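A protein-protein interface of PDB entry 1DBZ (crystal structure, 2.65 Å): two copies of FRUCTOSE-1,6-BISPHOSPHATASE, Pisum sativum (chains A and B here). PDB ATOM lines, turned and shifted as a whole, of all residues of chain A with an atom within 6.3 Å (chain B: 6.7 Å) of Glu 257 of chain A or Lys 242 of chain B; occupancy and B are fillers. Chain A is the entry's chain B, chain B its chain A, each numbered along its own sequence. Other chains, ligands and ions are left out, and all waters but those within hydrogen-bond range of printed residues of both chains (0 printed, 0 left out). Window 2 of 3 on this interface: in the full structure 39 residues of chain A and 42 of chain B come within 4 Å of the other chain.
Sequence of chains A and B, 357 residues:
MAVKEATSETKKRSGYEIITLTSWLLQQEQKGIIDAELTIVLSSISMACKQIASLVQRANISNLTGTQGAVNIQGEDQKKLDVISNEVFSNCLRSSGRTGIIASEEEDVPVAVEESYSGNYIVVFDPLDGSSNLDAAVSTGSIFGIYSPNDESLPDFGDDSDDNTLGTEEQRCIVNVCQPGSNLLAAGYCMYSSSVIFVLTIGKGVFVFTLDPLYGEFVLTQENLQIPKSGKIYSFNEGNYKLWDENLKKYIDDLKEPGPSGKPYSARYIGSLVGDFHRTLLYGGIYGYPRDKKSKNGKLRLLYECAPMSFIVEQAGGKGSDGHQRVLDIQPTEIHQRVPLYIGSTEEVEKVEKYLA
NZ of Lys 242 of chain B lies within salt-bridge range of OE2 of Glu 257 of chain A (2.8 Å). The side-chain carboxylate (OE1) of Glu 238 of chain B is in salt-bridge range of the side-chain amino group (NZ) of Lys 256 of chain A (3.1 Å).
O of Leu 255 of chain A is in hydrogen-bond range of N of Tyr 265 of chain A (3.3 Å).
Among the printed residues, merely in contact across the chains: Lys 256 of chain A with Tyr 241 of chain B (3.8 Å), Lys 256 of chain A with Lys 242 of chain B (3.4 Å), Pro 264 of chain A with Gly 239 of chain B (3.1 Å) and Tyr 265 of chain A with Gly 239 of chain B (3.2 Å).
Of the printed residues of chain B, Lys 256 of chain A touches Glu 238, Tyr 241 and Lys 242. Glu 257 of chain A touches just one residue of chain B: Lys 242 (2.8 Å). Of the printed residues of chain B, Pro 264 of chain A touches Gly 239 (3.1 Å). Of the printed residues of chain B, Tyr 265 of chain A touches Gly 239 (3.2 Å). Printed residues of chain A within 4 Å of Tyr 241 of chain B: Lys 256 (3.8 Å). Lys 242 of chain B touches just these residues of chain A: Lys 256 and Glu 257. Trp 244 of chain B touches none of the printed residues of chain A. Lys 249 of chain B touches none of the printed residues of chain A. The nearest residue of chain B that does not touch Glu 257 of chain A is Gly 239 of chain B (5.8 Å). The nearest printed residue of chain A that does not touch Glu 238 of chain B is Tyr 265 of chain A (5.5 Å).
Of the 10 printed residues of chain B, 4 touch a printed residue of chain A. Hydrophobic or aromatic side chains of chain B within 4 Å of the printed part of chain A: Tyr 241. Printed residues of chain A that touch a printed residue of chain B: Lys 256, Glu 257, Pro 264 and Tyr 265. Hydrophobic or aromatic side chains of chain A that line the printed part of chain B: Pro 264. Among the printed residues, Asp or Glu carboxylates within 4 Å of a Lys or Arg side-chain nitrogen of the other chain: Lys 256 of chain A with Glu 238 of chain B and Glu 257 of chain A with Lys 242 of chain B.
No position is printed for both chains. Of the 6 pairs that touch across the chains among the printed residues, none has its exchanged pair printed and touching as well.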
ATOM      1  N   ILE A 252       8.439   0.312   9.019  1.00  0.00           N
ATOM      2  CA  ILE A 252       7.811   0.444  10.325  1.00  0.00           C
ATOM      3  C   ILE A 252       8.317  -0.610  11.288  1.00  0.00           C
ATOM      4  O   ILE A 252       8.659  -0.306  12.432  1.00  0.00           O
ATOM      5  CB  ILE A 252       6.268   0.369  10.214  1.00  0.00           C
ATOM      6  CG1 ILE A 252       5.732   1.589   9.449  1.00  0.00           C
ATOM      7  CG2 ILE A 252       5.638   0.313  11.577  1.00  0.00           C
ATOM      8  CD1 ILE A 252       6.074   2.939  10.094  1.00  0.00           C
ATOM      9  N   ASP A 253       8.423  -1.838  10.797  1.00  0.00           N
ATOM     10  CA  ASP A 253       8.892  -2.951  11.600  1.00  0.00           C
ATOM     11  C   ASP A 253      10.326  -2.824  12.043  1.00  0.00           C
ATOM     12  O   ASP A 253      10.628  -3.089  13.202  1.00  0.00           O
ATOM     13  CB  ASP A 253       8.685  -4.267  10.868  1.00  0.00           C
ATOM     14  CG  ASP A 253       7.216  -4.612  10.705  1.00  0.00           C
ATOM     15  OD1 ASP A 253       6.407  -4.305  11.616  1.00  0.00           O
ATOM     16  OD2 ASP A 253       6.856  -5.188   9.658  1.00  0.00           O
ATOM     17  N   ASP A 254      11.207  -2.383  11.154  1.00  0.00           N
ATOM     18  CA  ASP A 254      12.611  -2.247  11.517  1.00  0.00           C
ATOM     19  C   ASP A 254      12.871  -1.157  12.531  1.00  0.00           C
ATOM     20  O   ASP A 254      13.941  -1.098  13.129  1.00  0.00           O
ATOM     21  CB  ASP A 254      13.484  -2.058  10.280  1.00  0.00           C
ATOM     22  CG  ASP A 254      13.579  -3.322   9.436  1.00  0.00           C
ATOM     23  OD1 ASP A 254      13.179  -4.405   9.908  1.00  0.00           O
ATOM     24  OD2 ASP A 254      14.057  -3.242   8.288  1.00  0.00           O
ATOM     25  N   LEU A 255      11.891  -0.286  12.725  1.00  0.00           N
ATOM     26  CA  LEU A 255      12.044   0.782  13.696  1.00  0.00           C
ATOM     27  C   LEU A 255      11.876   0.243  15.108  1.00  0.00           C
ATOM     28  O   LEU A 255      12.558   0.697  16.016  1.00  0.00           O
ATOM     29  CB  LEU A 255      11.014   1.887  13.460  1.00  0.00           C
ATOM     30  CG  LEU A 255      11.068   2.659  12.149  1.00  0.00           C
ATOM     31  CD1 LEU A 255       9.966   3.680  12.140  1.00  0.00           C
ATOM     32  CD2 LEU A 255      12.413   3.323  11.990  1.00  0.00           C
ATOM     33  N   LYS A 256      10.995  -0.750  15.268  1.00  0.00           N
ATOM     34  CA  LYS A 256      10.674  -1.363  16.560  1.00  0.00           C
ATOM     35  C   LYS A 256      11.731  -2.276  17.116  1.00  0.00           C
ATOM     36  O   LYS A 256      11.612  -2.753  18.234  1.00  0.00           O
ATOM     37  CB  LYS A 256       9.352  -2.097  16.458  1.00  0.00           C
ATOM     38  CG  LYS A 256       8.307  -1.238  15.798  1.00  0.00           C
ATOM     39  CD  LYS A 256       6.950  -1.855  15.852  1.00  0.00           C
ATOM     40  CE  LYS A 256       5.910  -0.903  15.291  1.00  0.00           C
ATOM     41  NZ  LYS A 256       4.547  -1.444  15.525  1.00  0.00           N
ATOM     42  N   GLU A 257      12.775  -2.487  16.329  1.00  0.00           N
ATOM     43  CA  GLU A 257      13.914  -3.321  16.697  1.00  0.00           C
ATOM     44  C   GLU A 257      14.873  -2.594  17.638  1.00  0.00           C
ATOM     45  O   GLU A 257      15.559  -1.644  17.230  1.00  0.00           O
ATOM     46  CB  GLU A 257      14.686  -3.730  15.442  1.00  0.00           C
ATOM     47  CG  GLU A 257      14.245  -5.050  14.821  1.00  0.00           C
ATOM     48  CD  GLU A 257      14.565  -6.267  15.694  1.00  0.00           C
ATOM     49  OE1 GLU A 257      15.669  -6.337  16.301  1.00  0.00           O
ATOM     50  OE2 GLU A 257      13.705  -7.165  15.764  1.00  0.00           O
ATOM     51  N   PRO A 258      14.943  -3.039  18.910  1.00  0.00           N
ATOM     52  CA  PRO A 258      15.836  -2.406  19.885  1.00  0.00           C
ATOM     53  C   PRO A 258      17.238  -2.457  19.334  1.00  0.00           C
ATOM     54  O   PRO A 258      17.878  -3.502  19.291  1.00  0.00           O
ATOM     55  CB  PRO A 258      15.654  -3.272  21.135  1.00  0.00           C
ATOM     56  CG  PRO A 258      15.191  -4.593  20.594  1.00  0.00           C
ATOM     57  CD  PRO A 258      14.232  -4.174  19.518  1.00  0.00           C
ATOM     58  N   GLY A 259      17.675  -1.319  18.819  1.00  0.00           N
ATOM     59  CA  GLY A 259      18.980  -1.252  18.238  1.00  0.00           C
ATOM     60  C   GLY A 259      20.124  -1.416  19.214  1.00  0.00           C
ATOM     61  O   GLY A 259      20.058  -2.218  20.163  1.00  0.00           O
ATOM     62  N   PRO A 260      21.096  -0.519  19.100  1.00  0.00           N
ATOM     63  CA  PRO A 260      22.322  -0.363  19.874  1.00  0.00           C
ATOM     64  C   PRO A 260      22.157  -0.710  21.331  1.00  0.00           C
ATOM     65  O   PRO A 260      22.195  -1.883  21.716  1.00  0.00           O
ATOM     66  CB  PRO A 260      22.694   1.095  19.669  1.00  0.00           C
ATOM     67  CG  PRO A 260      21.363   1.749  19.396  1.00  0.00           C
ATOM     68  CD  PRO A 260      20.795   0.775  18.430  1.00  0.00           C
ATOM     69  N   LYS A 263      17.531   0.071  22.504  1.00  0.00           N
ATOM     70  CA  LYS A 263      16.467   1.047  22.591  1.00  0.00           C
ATOM     71  C   LYS A 263      15.910   1.287  21.203  1.00  0.00           C
ATOM     72  O   LYS A 263      16.610   1.776  20.329  1.00  0.00           O
ATOM     73  CB  LYS A 263      16.991   2.323  23.172  1.00  0.00           C
ATOM     74  N   PRO A 264      14.657   0.880  20.966  1.00  0.00           N
ATOM     75  CA  PRO A 264      14.000   1.057  19.675  1.00  0.00           C
ATOM     76  C   PRO A 264      13.619   2.526  19.496  1.00  0.00           C
ATOM     77  O   PRO A 264      14.042   3.390  20.270  1.00  0.00           O
ATOM     78  CB  PRO A 264      12.761   0.193  19.819  1.00  0.00           C
ATOM     79  CG  PRO A 264      12.423   0.383  21.222  1.00  0.00           C
ATOM     80  CD  PRO A 264      13.741   0.242  21.918  1.00  0.00           C
ATOM     81  N   TYR A 265      12.814   2.818  18.488  1.00  0.00           N
ATOM     82  CA  TYR A 265      12.404   4.186  18.249  1.00  0.00           C
ATOM     83  C   TYR A 265      11.262   4.554  19.165  1.00  0.00           C
ATOM     84  O   TYR A 265      10.619   3.683  19.747  1.00  0.00           O
ATOM     85  CB  TYR A 265      11.937   4.355  16.808  1.00  0.00           C
ATOM     86  CG  TYR A 265      13.016   4.729  15.835  1.00  0.00           C
ATOM     87  CD1 TYR A 265      14.220   4.051  15.807  1.00  0.00           C
ATOM     88  CD2 TYR A 265      12.816   5.758  14.931  1.00  0.00           C
ATOM     89  CE1 TYR A 265      15.202   4.388  14.890  1.00  0.00           C
ATOM     90  CE2 TYR A 265      13.781   6.106  14.009  1.00  0.00           C
ATOM     91  CZ  TYR A 265      14.975   5.422  13.987  1.00  0.00           C
ATOM     92  OH  TYR A 265      15.931   5.762  13.043  1.00  0.00           O
ATOM     93  N   GLU B 238       3.823   2.435  20.539  1.00  0.00           N
ATOM     94  CA  GLU B 238       4.235   1.240  19.834  1.00  0.00           C
ATOM     95  C   GLU B 238       5.716   1.119  19.593  1.00  0.00           C
ATOM     96  O   GLU B 238       6.165   0.104  19.107  1.00  0.00           O
ATOM     97  CB  GLU B 238       3.493   1.098  18.522  1.00  0.00           C
ATOM     98  CG  GLU B 238       2.017   0.880  18.700  1.00  0.00           C
ATOM     99  CD  GLU B 238       1.363   0.212  17.507  1.00  0.00           C
ATOM    100  OE1 GLU B 238       1.904  -0.818  17.038  1.00  0.00           O
ATOM    101  OE2 GLU B 238       0.295   0.699  17.057  1.00  0.00           O
ATOM    102  N   GLY B 239       6.491   2.132  19.937  1.00  0.00           N
ATOM    103  CA  GLY B 239       7.918   2.011  19.719  1.00  0.00           C
ATOM    104  C   GLY B 239       8.446   0.862  20.554  1.00  0.00           C
ATOM    105  O   GLY B 239       9.447   0.226  20.213  1.00  0.00           O
ATOM    106  N   ASN B 240       7.724   0.562  21.629  1.00  0.00           N
ATOM    107  CA  ASN B 240       8.106  -0.496  22.553  1.00  0.00           C
ATOM    108  C   ASN B 240       7.445  -1.819  22.229  1.00  0.00           C
ATOM    109  O   ASN B 240       7.463  -2.733  23.044  1.00  0.00           O
ATOM    110  CB  ASN B 240       7.715  -0.114  23.975  1.00  0.00           C
ATOM    111  CG  ASN B 240       8.405   1.122  24.458  1.00  0.00           C
ATOM    112  OD1 ASN B 240       7.954   1.739  25.412  1.00  0.00           O
ATOM    113  ND2 ASN B 240       9.512   1.494  23.818  1.00  0.00           N
ATOM    114  N   TYR B 241       6.853  -1.926  21.053  1.00  0.00           N
ATOM    115  CA  TYR B 241       6.171  -3.148  20.683  1.00  0.00           C
ATOM    116  C   TYR B 241       6.958  -4.421  20.942  1.00  0.00           C
ATOM    117  O   TYR B 241       6.394  -5.416  21.390  1.00  0.00           O
ATOM    118  CB  TYR B 241       5.768  -3.088  19.233  1.00  0.00           C
ATOM    119  CG  TYR B 241       5.054  -4.319  18.761  1.00  0.00           C
ATOM    120  CD1 TYR B 241       3.710  -4.530  19.062  1.00  0.00           C
ATOM    121  CD2 TYR B 241       5.706  -5.254  17.961  1.00  0.00           C
ATOM    122  CE1 TYR B 241       3.031  -5.639  18.565  1.00  0.00           C
ATOM    123  CE2 TYR B 241       5.044  -6.362  17.463  1.00  0.00           C
ATOM    124  CZ  TYR B 241       3.714  -6.553  17.763  1.00  0.00           C
ATOM    125  OH  TYR B 241       3.076  -7.658  17.248  1.00  0.00           O
ATOM    126  N   LYS B 242       8.261  -4.385  20.681  1.00  0.00           N
ATOM    127  CA  LYS B 242       9.101  -5.563  20.880  1.00  0.00           C
ATOM    128  C   LYS B 242       9.530  -5.833  22.314  1.00  0.00           C
ATOM    129  O   LYS B 242      10.213  -6.819  22.591  1.00  0.00           O
ATOM    130  CB  LYS B 242      10.294  -5.546  19.918  1.00  0.00           C
ATOM    131  CG  LYS B 242       9.821  -5.681  18.476  1.00  0.00           C
ATOM    132  CD  LYS B 242      10.849  -6.212  17.508  1.00  0.00           C
ATOM    133  CE  LYS B 242      10.153  -6.519  16.173  1.00  0.00           C
ATOM    134  NZ  LYS B 242      11.061  -6.758  15.000  1.00  0.00           N
ATOM    135  N   LEU B 243       9.087  -4.981  23.231  1.00  0.00           N
ATOM    136  CA  LEU B 243       9.415  -5.141  24.637  1.00  0.00           C
ATOM    137  C   LEU B 243       8.192  -5.638  25.407  1.00  0.00           C
ATOM    138  O   LEU B 243       8.281  -5.962  26.597  1.00  0.00           O
ATOM    139  CB  LEU B 243       9.873  -3.815  25.240  1.00  0.00           C
ATOM    140  CG  LEU B 243      10.968  -3.004  24.544  1.00  0.00           C
ATOM    141  CD1 LEU B 243      11.417  -1.871  25.467  1.00  0.00           C
ATOM    142  CD2 LEU B 243      12.156  -3.887  24.185  1.00  0.00           C
ATOM    143  N   TRP B 244       7.050  -5.682  24.726  1.00  0.00           N
ATOM    144  CA  TRP B 244       5.797  -6.113  25.326  1.00  0.00           C
ATOM    145  C   TRP B 244       5.630  -7.635  25.374  1.00  0.00           C
ATOM    146  O   TRP B 244       6.340  -8.378  24.688  1.00  0.00           O
ATOM    147  CB  TRP B 244       4.627  -5.493  24.570  1.00  0.00           C
ATOM    148  CG  TRP B 244       4.554  -4.018  24.694  1.00  0.00           C
ATOM    149  CD1 TRP B 244       5.178  -3.229  25.631  1.00  0.00           C
ATOM    150  CD2 TRP B 244       3.811  -3.135  23.859  1.00  0.00           C
ATOM    151  NE1 TRP B 244       4.864  -1.913  25.423  1.00  0.00           N
ATOM    152  CE2 TRP B 244       4.026  -1.824  24.338  1.00  0.00           C
ATOM    153  CE3 TRP B 244       2.985  -3.322  22.744  1.00  0.00           C
ATOM    154  CZ2 TRP B 244       3.439  -0.694  23.732  1.00  0.00           C
ATOM    155  CZ3 TRP B 244       2.402  -2.194  22.139  1.00  0.00           C
ATOM    156  CH2 TRP B 244       2.634  -0.903  22.638  1.00  0.00           C
ATOM    157  N   ASP B 245       4.699  -8.095  26.205  1.00  0.00           N
ATOM    158  CA  ASP B 245       4.421  -9.519  26.331  1.00  0.00           C
ATOM    159  C   ASP B 245       3.695  -9.988  25.085  1.00  0.00           C
ATOM    160  O   ASP B 245       3.083  -9.171  24.384  1.00  0.00           O
ATOM    161  CB  ASP B 245       3.535  -9.778  27.551  1.00  0.00           C
ATOM    162  CG  ASP B 245       4.236  -9.477  28.868  1.00  0.00           C
ATOM    163  OD1 ASP B 245       5.424  -9.072  28.855  1.00  0.00           O
ATOM    164  OD2 ASP B 245       3.587  -9.651  29.926  1.00  0.00           O
ATOM    165  N   LYS B 249       1.116  -8.038  22.498  1.00  0.00           N
ATOM    166  CA  LYS B 249       1.420  -7.955  21.074  1.00  0.00           C
ATOM    167  C   LYS B 249       0.214  -8.371  20.248  1.00  0.00           C
ATOM    168  O   LYS B 249      -0.135  -7.710  19.277  1.00  0.00           O
ATOM    169  CB  LYS B 249       2.599  -8.832  20.710  1.00  0.00           C
ATOM    170  CG  LYS B 249       3.931  -8.339  21.203  1.00  0.00           C
ATOM    171  CD  LYS B 249       5.030  -9.129  20.509  1.00  0.00           C
ATOM    172  CE  LYS B 249       6.420  -8.797  21.041  1.00  0.00           C
ATOM    173  NZ  LYS B 249       7.486  -9.605  20.363  1.00  0.00           N
ATOM    174  N   LYS B 293       9.864  -5.450  29.069  1.00  0.00           N
ATOM    175  CA  LYS B 293      10.965  -6.278  29.555  1.00  0.00           C
ATOM    176  C   LYS B 293      11.714  -5.637  30.707  1.00  0.00           C
ATOM    177  O   LYS B 293      11.765  -6.178  31.821  1.00  0.00           O
ATOM    178  CB  LYS B 293      11.948  -6.629  28.425  1.00  0.00           C
ATOM    179  CG  LYS B 293      11.552  -7.851  27.576  1.00  0.00           C
ATOM    180  CD  LYS B 293      11.260  -9.092  28.454  1.00  0.00           C
ATOM    181  CE  LYS B 293      11.362 -10.438  27.698  1.00  0.00           C
ATOM    182  NZ  LYS B 293      12.762 -10.991  27.611  1.00  0.00           N
